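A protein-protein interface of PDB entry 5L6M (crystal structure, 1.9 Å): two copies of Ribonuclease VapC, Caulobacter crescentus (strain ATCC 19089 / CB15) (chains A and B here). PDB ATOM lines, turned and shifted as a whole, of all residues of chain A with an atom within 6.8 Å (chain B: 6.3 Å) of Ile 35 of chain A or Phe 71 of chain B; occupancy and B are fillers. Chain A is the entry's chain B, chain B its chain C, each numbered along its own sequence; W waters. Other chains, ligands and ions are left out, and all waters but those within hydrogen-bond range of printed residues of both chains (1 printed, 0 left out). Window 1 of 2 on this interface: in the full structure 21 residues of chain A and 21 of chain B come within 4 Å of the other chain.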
ATOM      1  N   LEU A  33       6.228  18.099  -5.814  1.00  0.00           N
ATOM      2  CA  LEU A  33       6.514  19.447  -6.291  1.00  0.00           C
ATOM      3  C   LEU A  33       7.889  19.492  -6.933  1.00  0.00           C
ATOM      4  O   LEU A  33       8.874  19.077  -6.323  1.00  0.00           O
ATOM      5  CB  LEU A  33       6.460  20.467  -5.155  1.00  0.00           C
ATOM      6  CG  LEU A  33       6.442  21.910  -5.646  1.00  0.00           C
ATOM      7  CD1 LEU A  33       5.043  22.238  -6.172  1.00  0.00           C
ATOM      8  CD2 LEU A  33       6.840  22.854  -4.519  1.00  0.00           C
ATOM      9  N   SER A  34       7.954  19.997  -8.155  1.00  0.00           N
ATOM     10  CA  SER A  34       9.242  20.224  -8.787  1.00  0.00           C
ATOM     11  C   SER A  34       9.987  21.372  -8.099  1.00  0.00           C
ATOM     12  O   SER A  34       9.397  22.404  -7.761  1.00  0.00           O
ATOM     13  CB  SER A  34       9.033  20.544 -10.264  1.00  0.00           C
ATOM     14  OG  SER A  34      10.168  21.192 -10.800  1.00  0.00           O
ATOM     15  N   ILE A  35      11.307  21.215  -7.935  1.00  0.00           N
ATOM     16  CA  ILE A  35      12.116  22.321  -7.424  1.00  0.00           C
ATOM     17  C   ILE A  35      12.033  23.509  -8.357  1.00  0.00           C
ATOM     18  O   ILE A  35      12.233  24.654  -7.926  1.00  0.00           O
ATOM     19  CB  ILE A  35      13.584  21.901  -7.228  1.00  0.00           C
ATOM     20  CG1 ILE A  35      14.368  22.966  -6.494  1.00  0.00           C
ATOM     21  CG2 ILE A  35      14.256  21.614  -8.575  1.00  0.00           C
ATOM     22  CD1 ILE A  35      14.533  22.708  -5.048  1.00  0.00           C
ATOM     23  N   ILE A  36      11.721  23.261  -9.637  1.00  0.00           N
ATOM     24  CA  ILE A  36      11.571  24.354 -10.589  1.00  0.00           C
ATOM     25  C   ILE A  36      10.318  25.163 -10.247  1.00  0.00           C
ATOM     26  O   ILE A  36      10.330  26.395 -10.264  1.00  0.00           O
ATOM     27  CB  ILE A  36      11.528  23.815 -12.026  1.00  0.00           C
ATOM     28  CG1 ILE A  36      12.780  22.960 -12.332  1.00  0.00           C
ATOM     29  CG2 ILE A  36      11.406  24.989 -13.056  1.00  0.00           C
ATOM     30  CD1 ILE A  36      14.110  23.716 -12.216  1.00  0.00           C
ATOM     31  N   SER A  37       9.234  24.475  -9.887  1.00  0.00           N
ATOM     32  CA  SER A  37       8.058  25.177  -9.376  1.00  0.00           C
ATOM     33  C   SER A  37       8.362  25.907  -8.079  1.00  0.00           C
ATOM     34  O   SER A  37       7.879  27.039  -7.862  1.00  0.00           O
ATOM     35  CB  SER A  37       6.924  24.173  -9.169  1.00  0.00           C
ATOM     36  OG  SER A  37       6.585  23.567 -10.402  1.00  0.00           O
ATOM     37  N   ARG A  38       9.191  25.295  -7.205  1.00  0.00           N
ATOM     38  CA  ARG A  38       9.522  25.977  -5.955  1.00  0.00           C
ATOM     39  C   ARG A  38      10.196  27.305  -6.244  1.00  0.00           C
ATOM     40  O   ARG A  38       9.889  28.318  -5.605  1.00  0.00           O
ATOM     41  CB  ARG A  38      10.429  25.134  -5.048  1.00  0.00           C
ATOM     42  CG  ARG A  38      10.822  25.959  -3.780  1.00  0.00           C
ATOM     43  CD  ARG A  38      11.735  25.269  -2.788  1.00  0.00           C
ATOM     44  NE  ARG A  38      12.396  26.299  -1.974  1.00  0.00           N
ATOM     45  CZ  ARG A  38      13.525  26.127  -1.296  1.00  0.00           C
ATOM     46  NH1 ARG A  38      14.132  24.943  -1.269  1.00  0.00           N
ATOM     47  NH2 ARG A  38      14.029  27.144  -0.604  1.00  0.00           N
ATOM     48  N   VAL A  39      11.139  27.312  -7.189  1.00  0.00           N
ATOM     49  CA  VAL A  39      11.813  28.556  -7.549  1.00  0.00           C
ATOM     50  C   VAL A  39      10.802  29.597  -8.023  1.00  0.00           C
ATOM     51  O   VAL A  39      10.857  30.767  -7.625  1.00  0.00           O
ATOM     52  CB  VAL A  39      12.882  28.285  -8.618  1.00  0.00           C
ATOM     53  CG1 VAL A  39      13.332  29.590  -9.247  1.00  0.00           C
ATOM     54  CG2 VAL A  39      14.068  27.513  -7.984  1.00  0.00           C
ATOM     55  N   GLU A  40       9.872  29.185  -8.896  1.00  0.00           N
ATOM     56  CA  GLU A  40       8.845  30.109  -9.368  1.00  0.00           C
ATOM     57  C   GLU A  40       7.953  30.584  -8.228  1.00  0.00           C
ATOM     58  O   GLU A  40       7.611  31.773  -8.158  1.00  0.00           O
ATOM     59  CB  GLU A  40       8.020  29.438 -10.465  1.00  0.00           C
ATOM     60  CG  GLU A  40       8.839  29.271 -11.764  1.00  0.00           C
ATOM     61  CD  GLU A  40       8.018  28.718 -12.928  1.00  0.00           C
ATOM     62  OE1 GLU A  40       7.497  29.519 -13.745  1.00  0.00           O
ATOM     63  OE2 GLU A  40       7.876  27.478 -13.008  1.00  0.00           O
ATOM     64  N   VAL A  68       9.860  17.527  -2.688  1.00  0.00           N
ATOM     65  CA  VAL A  68      10.360  18.319  -3.804  1.00  0.00           C
ATOM     66  C   VAL A  68      11.260  17.447  -4.678  1.00  0.00           C
ATOM     67  O   VAL A  68      12.199  16.809  -4.179  1.00  0.00           O
ATOM     68  CB  VAL A  68      11.094  19.577  -3.301  1.00  0.00           C
ATOM     69  CG1 VAL A  68      11.783  20.322  -4.448  1.00  0.00           C
ATOM     70  CG2 VAL A  68      10.084  20.515  -2.601  1.00  0.00           C
ATOM     71  N   LEU A  69      10.981  17.426  -5.981  1.00  0.00           N
ATOM     72  CA  LEU A  69      11.850  16.756  -6.954  1.00  0.00           C
ATOM     73  C   LEU A  69      12.946  17.701  -7.420  1.00  0.00           C
ATOM     74  O   LEU A  69      12.664  18.707  -8.078  1.00  0.00           O
ATOM     75  CB  LEU A  69      11.076  16.293  -8.182  1.00  0.00           C
ATOM     76  CG  LEU A  69      10.160  15.094  -8.099  1.00  0.00           C
ATOM     77  CD1 LEU A  69       9.335  15.093  -9.386  1.00  0.00           C
ATOM     78  CD2 LEU A  69      10.988  13.808  -7.993  1.00  0.00           C
ATOM     79  N   ASP A  70      14.195  17.356  -7.131  1.00  0.00           N
ATOM     80  CA  ASP A  70      15.281  18.154  -7.661  1.00  0.00           C
ATOM     81  C   ASP A  70      15.351  17.963  -9.172  1.00  0.00           C
ATOM     82  O   ASP A  70      14.765  17.026  -9.725  1.00  0.00           O
ATOM     83  CB  ASP A  70      16.608  17.775  -6.993  1.00  0.00           C
ATOM     84  CG  ASP A  70      16.684  18.265  -5.542  1.00  0.00           C
ATOM     85  OD1 ASP A  70      15.769  18.989  -5.121  1.00  0.00           O
ATOM     86  OD2 ASP A  70      17.641  17.935  -4.840  1.00  0.00           O
ATOM     87  N   PHE A  71      16.035  18.895  -9.850  1.00  0.00           N
ATOM     88  CA  PHE A  71      16.236  18.802 -11.296  1.00  0.00           C
ATOM     89  C   PHE A  71      17.628  18.233 -11.528  1.00  0.00           C
ATOM     90  O   PHE A  71      18.635  18.910 -11.278  1.00  0.00           O
ATOM     91  CB  PHE A  71      16.097  20.134 -12.032  1.00  0.00           C
ATOM     92  CG  PHE A  71      15.934  19.943 -13.526  1.00  0.00           C
ATOM     93  CD1 PHE A  71      14.697  19.676 -14.060  1.00  0.00           C
ATOM     94  CD2 PHE A  71      17.028  19.946 -14.365  1.00  0.00           C
ATOM     95  CE1 PHE A  71      14.538  19.441 -15.417  1.00  0.00           C
ATOM     96  CE2 PHE A  71      16.891  19.714 -15.722  1.00  0.00           C
ATOM     97  CZ  PHE A  71      15.636  19.457 -16.250  1.00  0.00           C
ATOM     98  N   ASP A  72      17.681  16.984 -11.997  1.00  0.00           N
ATOM     99  CA  ASP A  72      18.960  16.284 -12.039  1.00  0.00           C
ATOM    100  C   ASP A  72      19.207  15.697 -13.421  1.00  0.00           C
ATOM    101  O   ASP A  72      18.444  15.953 -14.346  1.00  0.00           O
ATOM    102  CB  ASP A  72      18.979  15.167 -10.985  1.00  0.00           C
ATOM    103  CG  ASP A  72      17.767  14.253 -11.093  1.00  0.00           C
ATOM    104  OD1 ASP A  72      17.064  14.295 -12.128  1.00  0.00           O
ATOM    105  OD2 ASP A  72      17.518  13.486 -10.147  1.00  0.00           O
ATOM    106  N   MET A  97      10.890  21.336 -18.773  1.00  0.00           N
ATOM    107  CA  MET A  97      11.732  20.866 -17.671  1.00  0.00           C
ATOM    108  C   MET A  97      10.885  20.219 -16.581  1.00  0.00           C
ATOM    109  O   MET A  97      11.238  19.156 -16.054  1.00  0.00           O
ATOM    110  CB  MET A  97      12.545  22.020 -17.082  1.00  0.00           C
ATOM    111  CG  MET A  97      13.653  22.568 -17.988  1.00  0.00           C
ATOM    112  SD  MET A  97      14.539  23.951 -17.194  1.00  0.00           S
ATOM    113  CE  MET A  97      14.973  23.194 -15.636  1.00  0.00           C
ATOM    114  N   GLN A 101      10.640  16.071 -15.442  1.00  0.00           N
ATOM    115  CA  GLN A 101      10.714  15.461 -14.117  1.00  0.00           C
ATOM    116  C   GLN A 101       9.572  14.484 -13.905  1.00  0.00           C
ATOM    117  O   GLN A 101       9.772  13.413 -13.316  1.00  0.00           O
ATOM    118  CB  GLN A 101      10.700  16.530 -13.041  1.00  0.00           C
ATOM    119  CG  GLN A 101      11.942  17.384 -13.059  1.00  0.00           C
ATOM    120  CD  GLN A 101      11.848  18.478 -12.067  1.00  0.00           C
ATOM    121  OE1 GLN A 101      11.189  19.484 -12.313  1.00  0.00           O
ATOM    122  NE2 GLN A 101      12.476  18.287 -10.910  1.00  0.00           N
ATOM    123  N   SER B  34      26.077  24.464 -14.708  1.00  0.00           N
ATOM    124  CA  SER B  34      24.737  24.276 -14.165  1.00  0.00           C
ATOM    125  C   SER B  34      23.906  23.355 -15.057  1.00  0.00           C
ATOM    126  O   SER B  34      23.961  23.423 -16.292  1.00  0.00           O
ATOM    127  CB  SER B  34      24.042  25.635 -14.005  1.00  0.00           C
ATOM    128  OG  SER B  34      22.625  25.520 -13.997  1.00  0.00           O
ATOM    129  N   ILE B  35      23.099  22.500 -14.421  1.00  0.00           N
ATOM    130  CA  ILE B  35      22.162  21.688 -15.197  1.00  0.00           C
ATOM    131  C   ILE B  35      21.198  22.572 -15.980  1.00  0.00           C
ATOM    132  O   ILE B  35      20.690  22.154 -17.032  1.00  0.00           O
ATOM    133  CB  ILE B  35      21.436  20.690 -14.268  1.00  0.00           C
ATOM    134  CG1 ILE B  35      20.676  19.636 -15.070  1.00  0.00           C
ATOM    135  CG2 ILE B  35      20.524  21.450 -13.286  1.00  0.00           C
ATOM    136  CD1 ILE B  35      20.938  18.231 -14.644  1.00  0.00           C
ATOM    137  N   ILE B  36      20.910  23.792 -15.491  1.00  0.00           N
ATOM    138  CA  ILE B  36      20.093  24.686 -16.295  1.00  0.00           C
ATOM    139  C   ILE B  36      20.819  24.999 -17.604  1.00  0.00           C
ATOM    140  O   ILE B  36      20.229  24.989 -18.694  1.00  0.00           O
ATOM    141  CB  ILE B  36      19.738  25.965 -15.513  1.00  0.00           C
ATOM    142  CG1 ILE B  36      19.074  25.638 -14.162  1.00  0.00           C
ATOM    143  CG2 ILE B  36      18.833  26.847 -16.329  1.00  0.00           C
ATOM    144  CD1 ILE B  36      17.924  24.685 -14.251  1.00  0.00           C
ATOM    145  N   LEU B  69      25.977  20.424 -12.281  1.00  0.00           N
ATOM    146  CA  LEU B  69      25.393  20.616 -10.943  1.00  0.00           C
ATOM    147  C   LEU B  69      23.880  20.415 -10.996  1.00  0.00           C
ATOM    148  O   LEU B  69      23.190  21.138 -11.717  1.00  0.00           O
ATOM    149  CB  LEU B  69      25.703  22.030 -10.430  1.00  0.00           C
ATOM    150  CG  LEU B  69      27.166  22.444 -10.438  1.00  0.00           C
ATOM    151  CD1 LEU B  69      27.355  23.832  -9.814  1.00  0.00           C
ATOM    152  CD2 LEU B  69      27.935  21.392  -9.654  1.00  0.00           C
ATOM    153  N   ASP B  70      23.366  19.437 -10.248  1.00  0.00           N
ATOM    154  CA  ASP B  70      21.923  19.226 -10.191  1.00  0.00           C
ATOM    155  C   ASP B  70      21.298  20.382  -9.425  1.00  0.00           C
ATOM    156  O   ASP B  70      21.899  20.885  -8.474  1.00  0.00           O
ATOM    157  CB  ASP B  70      21.603  17.901  -9.476  1.00  0.00           C
ATOM    158  CG  ASP B  70      22.089  16.684 -10.250  1.00  0.00           C
ATOM    159  OD1 ASP B  70      21.946  16.671 -11.486  1.00  0.00           O
ATOM    160  OD2 ASP B  70      22.649  15.767  -9.629  1.00  0.00           O
ATOM    161  N   PHE B  71      20.101  20.814  -9.845  1.00  0.00           N
ATOM    162  CA  PHE B  71      19.448  21.937  -9.178  1.00  0.00           C
ATOM    163  C   PHE B  71      18.714  21.418  -7.954  1.00  0.00           C
ATOM    164  O   PHE B  71      17.667  20.773  -8.084  1.00  0.00           O
ATOM    165  CB  PHE B  71      18.484  22.703 -10.089  1.00  0.00           C
ATOM    166  CG  PHE B  71      18.162  24.063  -9.552  1.00  0.00           C
ATOM    167  CD1 PHE B  71      17.160  24.239  -8.608  1.00  0.00           C
ATOM    168  CD2 PHE B  71      18.905  25.185  -9.953  1.00  0.00           C
ATOM    169  CE1 PHE B  71      16.884  25.525  -8.094  1.00  0.00           C
ATOM    170  CE2 PHE B  71      18.647  26.432  -9.433  1.00  0.00           C
ATOM    171  CZ  PHE B  71      17.636  26.606  -8.509  1.00  0.00           C
ATOM    172  N   ASP B  72      19.249  21.719  -6.767  1.00  0.00           N
ATOM    173  CA  ASP B  72      18.841  21.089  -5.501  1.00  0.00           C
ATOM    174  C   ASP B  72      18.251  22.121  -4.536  1.00  0.00           C
ATOM    175  O   ASP B  72      18.189  23.316  -4.836  1.00  0.00           O
ATOM    176  CB  ASP B  72      20.025  20.382  -4.842  1.00  0.00           C
ATOM    177  CG  ASP B  72      21.224  21.299  -4.617  1.00  0.00           C
ATOM    178  OD1 ASP B  72      21.154  22.512  -4.903  1.00  0.00           O
ATOM    179  OD2 ASP B  72      22.261  20.796  -4.147  1.00  0.00           O
ATOM    180  N   GLY B  73      17.806  21.630  -3.366  1.00  0.00           N
ATOM    181  CA  GLY B  73      17.290  22.524  -2.336  1.00  0.00           C
ATOM    182  C   GLY B  73      18.249  23.650  -1.991  1.00  0.00           C
ATOM    183  O   GLY B  73      17.828  24.789  -1.792  1.00  0.00           O
ATOM    184  N   ALA B  74      19.554  23.354  -1.932  1.00  0.00           N
ATOM    185  CA  ALA B  74      20.516  24.398  -1.592  1.00  0.00           C
ATOM    186  C   ALA B  74      20.527  25.490  -2.649  1.00  0.00           C
ATOM    187  O   ALA B  74      20.638  26.679  -2.323  1.00  0.00           O
ATOM    188  CB  ALA B  74      21.916  23.802  -1.414  1.00  0.00           C
ATOM    189  N   ALA B  75      20.376  25.118  -3.927  1.00  0.00           N
ATOM    190  CA  ALA B  75      20.316  26.163  -4.952  1.00  0.00           C
ATOM    191  C   ALA B  75      19.031  26.970  -4.836  1.00  0.00           C
ATOM    192  O   ALA B  75      19.040  28.185  -5.032  1.00  0.00           O
ATOM    193  CB  ALA B  75      20.435  25.570  -6.355  1.00  0.00           C
ATOM    194  N   ALA B  76      17.909  26.316  -4.534  1.00  0.00           N
ATOM    195  CA  ALA B  76      16.669  27.078  -4.402  1.00  0.00           C
ATOM    196  C   ALA B  76      16.700  27.996  -3.173  1.00  0.00           C
ATOM    197  O   ALA B  76      16.095  29.076  -3.196  1.00  0.00           O
ATOM    198  CB  ALA B  76      15.470  26.134  -4.350  1.00  0.00           C
ATOM    199  N   TYR B  79      18.415  30.938  -4.391  1.00  0.00           N
ATOM    200  CA  TYR B  79      17.481  31.694  -5.223  1.00  0.00           C
ATOM    201  C   TYR B  79      16.542  32.538  -4.367  1.00  0.00           C
ATOM    202  O   TYR B  79      16.297  33.716  -4.659  1.00  0.00           O
ATOM    203  CB  TYR B  79      16.675  30.763  -6.128  1.00  0.00           C
ATOM    204  CG  TYR B  79      15.787  31.560  -7.060  1.00  0.00           C
ATOM    205  CD1 TYR B  79      16.250  31.988  -8.313  1.00  0.00           C
ATOM    206  CD2 TYR B  79      14.504  31.938  -6.671  1.00  0.00           C
ATOM    207  CE1 TYR B  79      15.440  32.758  -9.148  1.00  0.00           C
ATOM    208  CE2 TYR B  79      13.707  32.688  -7.482  1.00  0.00           C
ATOM    209  CZ  TYR B  79      14.172  33.101  -8.725  1.00  0.00           C
ATOM    210  OH  TYR B  79      13.355  33.880  -9.521  1.00  0.00           O
ATOM    211  N   ARG B  96      19.252  33.733 -12.690  1.00  0.00           N
ATOM    212  CA  ARG B  96      19.490  33.660 -11.256  1.00  0.00           C
ATOM    213  C   ARG B  96      19.508  32.219 -10.761  1.00  0.00           C
ATOM    214  O   ARG B  96      20.139  31.936  -9.734  1.00  0.00           O
ATOM    215  CB  ARG B  96      18.445  34.464 -10.488  1.00  0.00           C
ATOM    216  CG  ARG B  96      18.651  35.999 -10.602  1.00  0.00           C
ATOM    217  CD  ARG B  96      17.356  36.750 -10.347  1.00  0.00           C
ATOM    218  NE  ARG B  96      17.570  38.173 -10.067  1.00  0.00           N
ATOM    219  CZ  ARG B  96      16.654  38.999  -9.564  1.00  0.00           C
ATOM    220  NH1 ARG B  96      15.425  38.570  -9.298  1.00  0.00           N
ATOM    221  NH2 ARG B  96      16.963  40.270  -9.342  1.00  0.00           N
ATOM    222  N   MET B  97      18.789  31.314 -11.430  1.00  0.00           N
ATOM    223  CA  MET B  97      18.906  29.908 -11.045  1.00  0.00           C
ATOM    224  C   MET B  97      20.328  29.425 -11.265  1.00  0.00           C
ATOM    225  O   MET B  97      20.880  28.684 -10.446  1.00  0.00           O
ATOM    226  CB  MET B  97      17.947  29.025 -11.845  1.00  0.00           C
ATOM    227  CG  MET B  97      16.455  29.225 -11.531  1.00  0.00           C
ATOM    228  SD  MET B  97      15.476  27.908 -12.321  1.00  0.00           S
ATOM    229  CE  MET B  97      15.255  28.592 -13.943  1.00  0.00           C
ATOM    230  N   ILE B  98      20.930  29.843 -12.370  1.00  0.00           N
ATOM    231  CA  ILE B  98      22.311  29.471 -12.653  1.00  0.00           C
ATOM    232  C   ILE B  98      23.250  30.094 -11.619  1.00  0.00           C
ATOM    233  O   ILE B  98      24.134  29.413 -11.078  1.00  0.00           O
ATOM    234  CB  ILE B  98      22.675  29.872 -14.093  1.00  0.00           C
ATOM    235  CG1 ILE B  98      21.809  29.084 -15.106  1.00  0.00           C
ATOM    236  CG2 ILE B  98      24.171  29.644 -14.362  1.00  0.00           C
ATOM    237  CD1 ILE B  98      21.939  29.608 -16.558  1.00  0.00           C
ATOM    238  N   ALA B 100      22.463  31.075  -8.613  1.00  0.00           N
ATOM    239  CA  ALA B 100      22.224  30.428  -7.321  1.00  0.00           C
ATOM    240  C   ALA B 100      23.054  29.151  -7.168  1.00  0.00           C
ATOM    241  O   ALA B 100      23.495  28.809  -6.062  1.00  0.00           O
ATOM    242  CB  ALA B 100      20.743  30.096  -7.156  1.00  0.00           C
ATOM    243  N   GLN B 101      23.237  28.405  -8.250  1.00  0.00           N
ATOM    244  CA  GLN B 101      24.058  27.210  -8.140  1.00  0.00           C
ATOM    245  C   GLN B 101      25.502  27.591  -7.893  1.00  0.00           C
ATOM    246  O   GLN B 101      26.198  26.926  -7.122  1.00  0.00           O
ATOM    247  CB  GLN B 101      23.930  26.347  -9.401  1.00  0.00           C
ATOM    248  CG  GLN B 101      22.493  25.829  -9.628  1.00  0.00           C
ATOM    249  CD  GLN B 101      22.464  24.551 -10.454  1.00  0.00           C
ATOM    250  OE1 GLN B 101      22.402  24.595 -11.666  1.00  0.00           O
ATOM    251  NE2 GLN B 101      22.509  23.412  -9.791  1.00  0.00           N
HETATM  252  O   HOH W   1      10.861  33.144  -9.573  1.00  0.00           O
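Of the 17 printed residues of chain B, 9 touch a printed residue of chain A.
Among the printed residues, no Asp or Glu carboxylate lies within 4 Å of a Lys or Arg side-chain nitrogen of the other chain.
Ile 36 of chain A touches none of the printed residues of chain B.
Of the printed residues of chain B, Val 39 of chain A touches Phe 71 (3.4 Å), Tyr 79 (3.4 Å) and Met 97 (3.9 Å).
Of chain A, only Ile 35, Val 39, Asp 70 and Phe 71 come within 4 Å of Phe 71 of chain B.
Of the printed residues of chain A, Gly 73 of chain B touches Ile 35, Arg 38 and Asp 70.
Ala 75 of chain B touches none of the printed residues of chain A.
Of the printed residues of chain A, Ala 76 of chain B touches Ile 35 (3.6 Å) and Arg 38 (3.6 Å).
Of the printed residues of chain A, Tyr 79 of chain B touches Val 39.
The nearest residue of chain B that does not touch Ile 35 of chain A is Ala 74 of chain B (5.9 Å).
The nearest residue of chain A that does not touch Phe 71 of chain B is Ile 36 of chain A (4.8 Å).
Ile 35 of chain A touches Phe 71 of chain B, and with the chains exchanged Phe 71 of chain A touches Ile 35 of chain B.
Asp 70 of chain A touches Phe 71 of chain B, and with the chains exchanged Phe 71 of chain A touches Asp 70 of chain B.
Asp 70 of chain A touches Asp 72 of chain B, and with the chains exchanged Asp 72 of chain A touches Asp 70 of chain B.
Met 97 of chain A touches Ile 36 of chain B, but with the chains exchanged Ile 36 of chain A does not touch Met 97 of chain B (4.4 Å).
9 positions are printed for both chains.
O of Phe 71 of chain A sits at hydrogen-bond distance from N of Phe 71 of chain B.
Among the printed residues, merely in contact across the chains: Ile 35 of chain A with Phe 71 of chain B (3.5 Å), Ile 35 of chain A with Asp 72 of chain B (3.7 Å), Ile 35 of chain A with Gly 73 of chain B (3.8 Å), Ile 35 of chain A with Ala 76 of chain B (3.6 Å), Arg 38 of chain A with Gly 73 of chain B (3.7 Å), Arg 38 of chain A with Ala 76 of chain B (3.6 Å), Val 39 of chain A with Phe 71 of chain B (3.4 Å), Val 39 of chain A with Tyr 79 of chain B (3.4 Å), Val 39 of chain A with Met 97 of chain B (3.9 Å), Asp 70 of chain A with Phe 71 of chain B (3.4 Å), Asp 70 of chain A with Asp 72 of chain B (3.4 Å), Asp 70 of chain A with Gly 73 of chain B (3.8 Å), Phe 71 of chain A with Ile 35 of chain B (3.7 Å), Phe 71 of chain A with Asp 70 of chain B (3.5 Å), Asp 72 of chain A with Ile 35 of chain B (3.3 Å), Asp 72 of chain A with Asp 70 of chain B (3.1 Å) and Met 97 of chain A with Ile 36 of chain B (3.6 Å).
The backbone carbonyl oxygen (O) of Leu 69 of chain A is in hydrogen-bond range of the backbone NH (N) of Ile 35 of chain A (2.9 Å).
The side-chain hydroxyl (OG) of Ser 34 of chain B is in hydrogen-bond range of the backbone NH (N) of Ile 36 of chain B.
The backbone NH (N) of Ile 35 of chain B lies within hydrogen-bond range of the backbone carbonyl oxygen (O) of Leu 69 of chain B, 3.0 Å away.
The backbone carbonyl oxygen (O) of Asp 70 of chain B lies within hydrogen-bond range of the side-chain amide nitrogen (NE2) of Gln 101 of chain B (2.9 Å).
OD1 of Asp 72 of chain B sits close to N of Ala 74 of chain B.
The side-chain carboxylate (OD1) of Asp 72 of chain B sits at hydrogen-bond distance from the backbone NH (N) of Ala 75 of chain B (2.9 Å).
Water W1 bridges the side-chain hydroxyl of Tyr 79 of chain B (2.6 Å) and the backbone carbonyl oxygen of Val 39 of chain A (3.1 Å).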
